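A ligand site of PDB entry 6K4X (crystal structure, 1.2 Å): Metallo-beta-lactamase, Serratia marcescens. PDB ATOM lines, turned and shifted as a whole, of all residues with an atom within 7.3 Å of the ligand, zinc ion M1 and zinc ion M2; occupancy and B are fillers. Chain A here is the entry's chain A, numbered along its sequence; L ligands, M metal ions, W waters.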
ATOM      1  N   TRP A   5     -22.866   6.761   7.091  1.00  0.00           N
ATOM      2  CA  TRP A   5     -23.320   6.699   5.710  1.00  0.00           C
ATOM      3  C   TRP A   5     -24.173   7.885   5.331  1.00  0.00           C
ATOM      4  O   TRP A   5     -24.322   8.179   4.180  1.00  0.00           O
ATOM      5  CB  TRP A   5     -24.181   5.458   5.456  1.00  0.00           C
ATOM      6  CG  TRP A   5     -23.484   4.147   5.514  1.00  0.00           C
ATOM      7  CD1 TRP A   5     -22.146   3.919   5.539  1.00  0.00           C
ATOM      8  CD2 TRP A   5     -24.137   2.877   5.592  1.00  0.00           C
ATOM      9  NE1 TRP A   5     -21.919   2.563   5.579  1.00  0.00           N
ATOM     10  CE2 TRP A   5     -23.118   1.908   5.640  1.00  0.00           C
ATOM     11  CE3 TRP A   5     -25.478   2.472   5.641  1.00  0.00           C
ATOM     12  CZ2 TRP A   5     -23.408   0.546   5.708  1.00  0.00           C
ATOM     13  CZ3 TRP A   5     -25.760   1.127   5.711  1.00  0.00           C
ATOM     14  CH2 TRP A   5     -24.741   0.181   5.756  1.00  0.00           C
ATOM     15  N   ILE A  26     -20.308   7.529   2.305  1.00  0.00           N
ATOM     16  CA  ILE A  26     -20.696   6.899   1.025  1.00  0.00           C
ATOM     17  C   ILE A  26     -20.417   7.880  -0.093  1.00  0.00           C
ATOM     18  O   ILE A  26     -20.835   9.043  -0.019  1.00  0.00           O
ATOM     19  CB  ILE A  26     -22.169   6.463   0.993  1.00  0.00           C
ATOM     20  CG1 ILE A  26     -22.506   5.444   2.087  1.00  0.00           C
ATOM     21  CG2 ILE A  26     -22.514   5.923  -0.378  1.00  0.00           C
ATOM     22  CD1 ILE A  26     -21.903   4.083   1.879  1.00  0.00           C
ATOM     23  N   HIS A  72     -24.739  -0.071  -7.391  1.00  0.00           N
ATOM     24  CA  HIS A  72     -25.546  -1.212  -7.076  1.00  0.00           C
ATOM     25  C   HIS A  72     -26.636  -0.857  -6.083  1.00  0.00           C
ATOM     26  O   HIS A  72     -26.616   0.166  -5.401  1.00  0.00           O
ATOM     27  CB  HIS A  72     -24.703  -2.416  -6.598  1.00  0.00           C
ATOM     28  CG  HIS A  72     -24.165  -2.303  -5.216  1.00  0.00           C
ATOM     29  ND1 HIS A  72     -22.936  -1.786  -4.940  1.00  0.00           N
ATOM     30  CD2 HIS A  72     -24.691  -2.669  -4.014  1.00  0.00           C
ATOM     31  CE1 HIS A  72     -22.711  -1.856  -3.641  1.00  0.00           C
ATOM     32  NE2 HIS A  72     -23.797  -2.384  -3.012  1.00  0.00           N
ATOM     33  N   SER A  73     -27.618  -1.775  -6.003  1.00  0.00           N
ATOM     34  CA  SER A  73     -28.927  -1.542  -5.407  1.00  0.00           C
ATOM     35  C   SER A  73     -28.993  -2.049  -3.964  1.00  0.00           C
ATOM     36  O   SER A  73     -29.839  -2.898  -3.655  1.00  0.00           O
ATOM     37  CB  SER A  73     -29.951  -2.190  -6.288  1.00  0.00           C
ATOM     38  OG  SER A  73     -29.587  -3.532  -6.606  1.00  0.00           O
ATOM     39  N   HIS A  74     -28.133  -1.492  -3.099  1.00  0.00           N
ATOM     40  CA  HIS A  74     -28.281  -1.644  -1.657  1.00  0.00           C
ATOM     41  C   HIS A  74     -28.530  -0.264  -1.055  1.00  0.00           C
ATOM     42  O   HIS A  74     -28.212   0.762  -1.653  1.00  0.00           O
ATOM     43  CB  HIS A  74     -27.053  -2.269  -1.001  1.00  0.00           C
ATOM     44  CG  HIS A  74     -26.836  -3.688  -1.427  1.00  0.00           C
ATOM     45  ND1 HIS A  74     -25.621  -4.288  -1.425  1.00  0.00           N
ATOM     46  CD2 HIS A  74     -27.734  -4.613  -1.805  1.00  0.00           C
ATOM     47  CE1 HIS A  74     -25.783  -5.533  -1.822  1.00  0.00           C
ATOM     48  NE2 HIS A  74     -27.062  -5.758  -2.059  1.00  0.00           N
ATOM     49  N   GLU A  75     -29.141  -0.261   0.126  1.00  0.00           N
ATOM     50  CA  GLU A  75     -29.660   0.950   0.751  1.00  0.00           C
ATOM     51  C   GLU A  75     -28.586   2.014   0.965  1.00  0.00           C
ATOM     52  O   GLU A  75     -28.914   3.195   1.014  1.00  0.00           O
ATOM     53  CB  GLU A  75     -30.350   0.600   2.066  1.00  0.00           C
ATOM     54  CG  GLU A  75     -29.397   0.188   3.179  1.00  0.00           C
ATOM     55  CD  GLU A  75     -29.958  -0.086   4.575  1.00  0.00           C
ATOM     56  OE1 GLU A  75     -30.858   0.658   4.988  1.00  0.00           O
ATOM     57  OE2 GLU A  75     -29.471  -1.025   5.259  1.00  0.00           O
ATOM     58  N   ASP A  76     -27.336   1.627   1.188  1.00  0.00           N
ATOM     59  CA  ASP A  76     -26.293   2.598   1.462  1.00  0.00           C
ATOM     60  C   ASP A  76     -25.903   3.423   0.222  1.00  0.00           C
ATOM     61  O   ASP A  76     -25.474   4.567   0.385  1.00  0.00           O
ATOM     62  CB  ASP A  76     -25.073   1.958   2.102  1.00  0.00           C
ATOM     63  CG  ASP A  76     -24.422   0.799   1.376  1.00  0.00           C
ATOM     64  OD1 ASP A  76     -25.137   0.064   0.647  1.00  0.00           O
ATOM     65  OD2 ASP A  76     -23.204   0.615   1.580  1.00  0.00           O
ATOM     66  N   HIS A  77     -25.983   2.836  -0.974  1.00  0.00           N
ATOM     67  CA  HIS A  77     -25.605   3.555  -2.200  1.00  0.00           C
ATOM     68  C   HIS A  77     -26.829   4.118  -2.915  1.00  0.00           C
ATOM     69  O   HIS A  77     -26.725   5.131  -3.637  1.00  0.00           O
ATOM     70  CB  HIS A  77     -24.835   2.632  -3.145  1.00  0.00           C
ATOM     71  CG  HIS A  77     -23.703   1.969  -2.452  1.00  0.00           C
ATOM     72  ND1 HIS A  77     -22.514   2.622  -2.161  1.00  0.00           N
ATOM     73  CD2 HIS A  77     -23.621   0.750  -1.887  1.00  0.00           C
ATOM     74  CE1 HIS A  77     -21.758   1.783  -1.460  1.00  0.00           C
ATOM     75  NE2 HIS A  77     -22.412   0.652  -1.248  1.00  0.00           N
ATOM     76  N   ASP A 111     -29.354 -12.315  -4.307  1.00  0.00           N
ATOM     77  CA  ASP A 111     -28.321 -11.503  -3.647  1.00  0.00           C
ATOM     78  C   ASP A 111     -27.735 -12.318  -2.494  1.00  0.00           C
ATOM     79  O   ASP A 111     -28.491 -12.806  -1.659  1.00  0.00           O
ATOM     80  CB  ASP A 111     -28.942 -10.199  -3.159  1.00  0.00           C
ATOM     81  CG  ASP A 111     -27.938  -9.168  -2.673  1.00  0.00           C
ATOM     82  OD1 ASP A 111     -27.090  -9.503  -1.835  1.00  0.00           O
ATOM     83  OD2 ASP A 111     -28.036  -8.028  -3.154  1.00  0.00           O
ATOM     84  N   GLN A 113     -26.566 -11.414   0.218  1.00  0.00           N
ATOM     85  CA  GLN A 113     -27.014 -10.856   1.489  1.00  0.00           C
ATOM     86  C   GLN A 113     -28.514 -11.014   1.721  1.00  0.00           C
ATOM     87  O   GLN A 113     -29.005 -10.599   2.774  1.00  0.00           O
ATOM     88  CB  GLN A 113     -26.610  -9.386   1.586  1.00  0.00           C
ATOM     89  CG  GLN A 113     -25.123  -9.188   1.733  1.00  0.00           C
ATOM     90  CD  GLN A 113     -24.798  -7.723   1.885  1.00  0.00           C
ATOM     91  OE1 GLN A 113     -24.932  -7.150   2.971  1.00  0.00           O
ATOM     92  NE2 GLN A 113     -24.446  -7.053   0.804  1.00  0.00           N
ATOM     93  N   SER A 116     -30.760 -10.468   5.034  1.00  0.00           N
ATOM     94  CA  SER A 116     -30.076  -9.577   5.959  1.00  0.00           C
ATOM     95  C   SER A 116     -30.105  -8.125   5.460  1.00  0.00           C
ATOM     96  O   SER A 116     -29.560  -7.241   6.114  1.00  0.00           O
ATOM     97  CB  SER A 116     -28.666 -10.040   6.231  1.00  0.00           C
ATOM     98  OG  SER A 116     -27.830  -9.818   5.096  1.00  0.00           O
ATOM     99  N   LEU A 117     -30.756  -7.854   4.327  1.00  0.00           N
ATOM    100  CA  LEU A 117     -30.735  -6.512   3.737  1.00  0.00           C
ATOM    101  C   LEU A 117     -31.947  -5.705   4.216  1.00  0.00           C
ATOM    102  O   LEU A 117     -33.018  -6.269   4.431  1.00  0.00           O
ATOM    103  CB  LEU A 117     -30.742  -6.590   2.216  1.00  0.00           C
ATOM    104  CG  LEU A 117     -29.483  -7.171   1.594  1.00  0.00           C
ATOM    105  CD1 LEU A 117     -29.735  -7.635   0.163  1.00  0.00           C
ATOM    106  CD2 LEU A 117     -28.344  -6.162   1.652  1.00  0.00           C
ATOM    107  N   HIS A 150     -21.191  -8.792  -6.266  1.00  0.00           N
ATOM    108  CA  HIS A 150     -21.830  -8.242  -5.061  1.00  0.00           C
ATOM    109  C   HIS A 150     -23.349  -8.112  -5.267  1.00  0.00           C
ATOM    110  O   HIS A 150     -24.121  -8.339  -4.337  1.00  0.00           O
ATOM    111  CB  HIS A 150     -21.122  -6.974  -4.649  1.00  0.00           C
ATOM    112  CG  HIS A 150     -21.632  -6.305  -3.437  1.00  0.00           C
ATOM    113  ND1 HIS A 150     -21.205  -6.666  -2.187  1.00  0.00           N
ATOM    114  CD2 HIS A 150     -22.469  -5.264  -3.273  1.00  0.00           C
ATOM    115  CE1 HIS A 150     -21.761  -5.842  -1.300  1.00  0.00           C
ATOM    116  NE2 HIS A 150     -22.581  -4.994  -1.923  1.00  0.00           N
ATOM    117  N   THR A 151     -23.723  -7.744  -6.491  1.00  0.00           N
ATOM    118  CA  THR A 151     -25.090  -7.791  -6.976  1.00  0.00           C
ATOM    119  C   THR A 151     -25.022  -8.182  -8.447  1.00  0.00           C
ATOM    120  O   THR A 151     -23.995  -7.966  -9.103  1.00  0.00           O
ATOM    121  CB  THR A 151     -25.852  -6.449  -6.860  1.00  0.00           C
ATOM    122  OG1 THR A 151     -25.299  -5.500  -7.786  1.00  0.00           O
ATOM    123  CG2 THR A 151     -25.933  -5.902  -5.458  1.00  0.00           C
ATOM    124  N   ASP A 174     -17.669   0.280  -8.418  1.00  0.00           N
ATOM    125  CA  ASP A 174     -18.650  -0.464  -7.647  1.00  0.00           C
ATOM    126  C   ASP A 174     -17.932  -1.374  -6.653  1.00  0.00           C
ATOM    127  O   ASP A 174     -16.747  -1.692  -6.788  1.00  0.00           O
ATOM    128  CB  ASP A 174     -19.534  -1.301  -8.558  1.00  0.00           C
ATOM    129  CG  ASP A 174     -20.758  -1.862  -7.873  1.00  0.00           C
ATOM    130  OD1 ASP A 174     -21.129  -1.323  -6.832  1.00  0.00           O
ATOM    131  OD2 ASP A 174     -21.355  -2.796  -8.467  1.00  0.00           O
ATOM    132  N   SER A 175     -18.676  -1.769  -5.613  1.00  0.00           N
ATOM    133  CA  SER A 175     -18.223  -2.770  -4.635  1.00  0.00           C
ATOM    134  C   SER A 175     -18.024  -4.122  -5.293  1.00  0.00           C
ATOM    135  O   SER A 175     -18.865  -4.602  -6.034  1.00  0.00           O
ATOM    136  CB  SER A 175     -19.206  -2.860  -3.513  1.00  0.00           C
ATOM    137  OG  SER A 175     -19.376  -1.578  -2.930  1.00  0.00           O
ATOM    138  N   LEU A 176     -16.903  -4.764  -4.933  1.00  0.00           N
ATOM    139  CA  LEU A 176     -16.539  -6.086  -5.434  1.00  0.00           C
ATOM    140  C   LEU A 176     -16.466  -7.103  -4.296  1.00  0.00           C
ATOM    141  O   LEU A 176     -15.706  -8.075  -4.381  1.00  0.00           O
ATOM    142  CB  LEU A 176     -15.191  -5.994  -6.137  1.00  0.00           C
ATOM    143  CG  LEU A 176     -15.090  -4.989  -7.268  1.00  0.00           C
ATOM    144  CD1 LEU A 176     -13.695  -5.017  -7.870  1.00  0.00           C
ATOM    145  CD2 LEU A 176     -16.162  -5.222  -8.329  1.00  0.00           C
ATOM    146  N   THR A 177     -17.243  -6.872  -3.228  1.00  0.00           N
ATOM    147  CA  THR A 177     -17.065  -7.585  -1.975  1.00  0.00           C
ATOM    148  C   THR A 177     -18.001  -8.799  -1.884  1.00  0.00           C
ATOM    149  O   THR A 177     -19.218  -8.719  -2.039  1.00  0.00           O
ATOM    150  CB  THR A 177     -17.344  -6.628  -0.816  1.00  0.00           C
ATOM    151  OG1 THR A 177     -18.614  -6.034  -1.037  1.00  0.00           O
ATOM    152  CG2 THR A 177     -16.264  -5.578  -0.698  1.00  0.00           C
ATOM    153  N   ALA A 178     -17.408  -9.926  -1.499  1.00  0.00           N
ATOM    154  CA  ALA A 178     -18.112 -11.159  -1.162  1.00  0.00           C
ATOM    155  C   ALA A 178     -18.548 -11.067   0.299  1.00  0.00           C
ATOM    156  O   ALA A 178     -17.724 -11.129   1.250  1.00  0.00           O
ATOM    157  CB  ALA A 178     -17.209 -12.354  -1.381  1.00  0.00           C
ATOM    158  N   VAL A 179     -19.829 -10.813   0.503  1.00  0.00           N
ATOM    159  CA  VAL A 179     -20.440 -10.697   1.851  1.00  0.00           C
ATOM    160  C   VAL A 179     -21.819 -11.343   1.747  1.00  0.00           C
ATOM    161  O   VAL A 179     -22.433 -11.339   0.701  1.00  0.00           O
ATOM    162  CB  VAL A 179     -20.505  -9.214   2.290  1.00  0.00           C
ATOM    163  CG1 VAL A 179     -21.177  -8.361   1.242  1.00  0.00           C
ATOM    164  CG2 VAL A 179     -21.181  -8.959   3.634  1.00  0.00           C
ATOM    165  N   SER A 180     -22.284 -11.952   2.830  1.00  0.00           N
ATOM    166  CA  SER A 180     -23.541 -12.673   2.721  1.00  0.00           C
ATOM    167  C   SER A 180     -24.265 -12.746   4.049  1.00  0.00           C
ATOM    168  O   SER A 180     -23.706 -12.463   5.104  1.00  0.00           O
ATOM    169  CB  SER A 180     -23.309 -14.068   2.211  1.00  0.00           C
ATOM    170  OG  SER A 180     -22.765 -14.905   3.235  1.00  0.00           O
ATOM    171  N   ALA A 214     -17.118   3.239  -4.194  1.00  0.00           N
ATOM    172  CA  ALA A 214     -18.438   3.485  -3.673  1.00  0.00           C
ATOM    173  C   ALA A 214     -18.408   3.673  -2.145  1.00  0.00           C
ATOM    174  O   ALA A 214     -19.073   4.562  -1.599  1.00  0.00           O
ATOM    175  CB  ALA A 214     -19.368   2.372  -4.098  1.00  0.00           C
ATOM    176  N   HIS A 215     -17.655   2.824  -1.445  1.00  0.00           N
ATOM    177  CA  HIS A 215     -17.213   3.102  -0.083  1.00  0.00           C
ATOM    178  C   HIS A 215     -15.884   3.835  -0.163  1.00  0.00           C
ATOM    179  O   HIS A 215     -14.876   3.249  -0.553  1.00  0.00           O
ATOM    180  CB  HIS A 215     -17.078   1.819   0.741  1.00  0.00           C
ATOM    181  CG  HIS A 215     -18.408   1.222   1.084  1.00  0.00           C
ATOM    182  ND1 HIS A 215     -19.157   1.660   2.165  1.00  0.00           N
ATOM    183  CD2 HIS A 215     -19.175   0.303   0.447  1.00  0.00           C
ATOM    184  CE1 HIS A 215     -20.315   1.025   2.176  1.00  0.00           C
ATOM    185  NE2 HIS A 215     -20.358   0.183   1.142  1.00  0.00           N
ATOM    186  N   VAL A 218     -12.260   2.640   0.610  1.00  0.00           N
ATOM    187  CA  VAL A 218     -11.677   1.554  -0.108  1.00  0.00           C
ATOM    188  C   VAL A 218     -10.436   2.019  -0.887  1.00  0.00           C
ATOM    189  O   VAL A 218      -9.474   1.259  -1.005  1.00  0.00           O
ATOM    190  CB  VAL A 218     -12.721   0.884  -1.013  1.00  0.00           C
ATOM    191  CG1 VAL A 218     -12.099   0.020  -2.096  1.00  0.00           C
ATOM    192  CG2 VAL A 218     -13.677   0.067  -0.168  1.00  0.00           C
ATOM    193  N   ARG A 252     -10.680 -11.012  -0.524  1.00  0.00           N
ATOM    194  CA  ARG A 252     -11.836 -11.227   0.327  1.00  0.00           C
ATOM    195  C   ARG A 252     -12.579 -12.498  -0.112  1.00  0.00           C
ATOM    196  O   ARG A 252     -13.010 -13.284   0.744  1.00  0.00           O
ATOM    197  CB  ARG A 252     -12.756 -10.005   0.272  1.00  0.00           C
ATOM    198  CG  ARG A 252     -13.951 -10.078   1.190  1.00  0.00           C
ATOM    199  CD  ARG A 252     -14.666  -8.740   1.266  1.00  0.00           C
ATOM    200  NE  ARG A 252     -15.764  -8.794   2.215  1.00  0.00           N
ATOM    201  CZ  ARG A 252     -16.284  -7.771   2.856  1.00  0.00           C
ATOM    202  NH1 ARG A 252     -15.800  -6.557   2.674  1.00  0.00           N
ATOM    203  NH2 ARG A 252     -17.334  -7.968   3.631  1.00  0.00           N
HETATM  204  O1  LIG L   1     -20.741  -2.110  -0.685  1.00  0.00           O
HETATM  205  C1  LIG L   1     -20.142  -2.996  -0.030  1.00  0.00           C
HETATM  206  O2  LIG L   1     -18.978  -3.384  -0.346  1.00  0.00           O
HETATM  207  C2  LIG L   1     -20.778  -3.650   1.137  1.00  0.00           C
HETATM  208  C3  LIG L   1     -19.913  -4.451   1.951  1.00  0.00           C
HETATM  209  C4  LIG L   1     -22.129  -3.513   1.480  1.00  0.00           C
HETATM  210  S1  LIG L   1     -23.329  -2.541   0.743  1.00  0.00           S
HETATM  211  C5  LIG L   1     -22.594  -4.227   2.612  1.00  0.00           C
HETATM  212  C6  LIG L   1     -21.748  -5.027   3.399  1.00  0.00           C
HETATM  213  N1  LIG L   1     -22.233  -5.678   4.528  1.00  0.00           N
HETATM  214  C7  LIG L   1     -20.422  -5.101   3.074  1.00  0.00           C
HETATM  215 ZN    ZN M   1     -23.731  -3.462  -1.302  1.00  0.00          ZN
HETATM  216 ZN    ZN M   2     -22.073  -0.587   0.334  1.00  0.00          ZN
HETATM  217  O   HOH W   1     -16.529  -2.188  -1.003  1.00  0.00           O
HETATM  218  O   HOH W   2     -20.676  -7.445   6.443  1.00  0.00           O
HETATM  219  O   HOH W   3     -18.867  -1.695   3.619  1.00  0.00           O
HETATM  220  O   HOH W   4     -22.109  -1.247   3.700  1.00  0.00           O
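The side-chain hydroxyl (OG) of Ser 175 is in hydrogen-bond range of an oxygen (O2) of the ligand (3.2 Å). OG1 of Thr 177 lies within hydrogen-bond range of O2 of the ligand (2.8 Å). N1 of the ligand lies within hydrogen-bond range of OE1 of Gln 113, at 3.4 Å.
O of Thr 177 lies within hydrogen-bond range of ND1 of His 150 (2.9 Å). OD1 of Asp 174 is in hydrogen-bond range of ND1 of His 72 (2.7 Å). A ring nitrogen (NE2) of His 74 sits at hydrogen-bond distance from the side-chain carboxylate (OD2) of Asp 111 (2.7 Å). The side-chain carboxylate (OD1) of Asp 111 lies within hydrogen-bond range of the backbone NH (N) of Gln 113, at 2.9 Å. O of Gln 113 lies within hydrogen-bond range of OG of Ser 116.
Val 179 touches the ligand (CG2 to N1, 3.6 Å). Hydrophobic or aromatic side chains within 4 Å of the ligand: His 72, His 150, Val 179 and His 215. Within 4 Å of the ligand: His 72, His 74, Asp 76, His 77, Gln 113, His 150, Ser 175, Thr 177, Val 179 and His 215. The nearest printed residue that does not touch the ligand is Arg 252 (4.3 Å).
The nearest printed residue that does not touch zinc ion M1 is Gln 113 (4.2 Å).
NE2 of His 150 binds zinc ion M1 (2.0 Å). Zinc ion M1 is bound by NE2 of His 72, at 2.0 Å. Zinc ion M1 is bound by ND1 of His 74, 2.1 Å away. S1 of the ligand is bound to zinc ion M1. Zinc ion M1 has four donor atoms within binding distance.
Zinc ion M2 is bound by NE2 of His 77 (2.0 Å), NE2 of His 215 (2.0 Å), OD2 of Asp 76 (2.1 Å), O1 of the ligand (2.3 Å) and S1 of the ligand (2.4 Å). Zinc ion M2 has five donor atoms within binding distance.
Water W1 bridges O2 of the ligand (2.8 Å) and OG of Ser 175 (3.5 Å).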
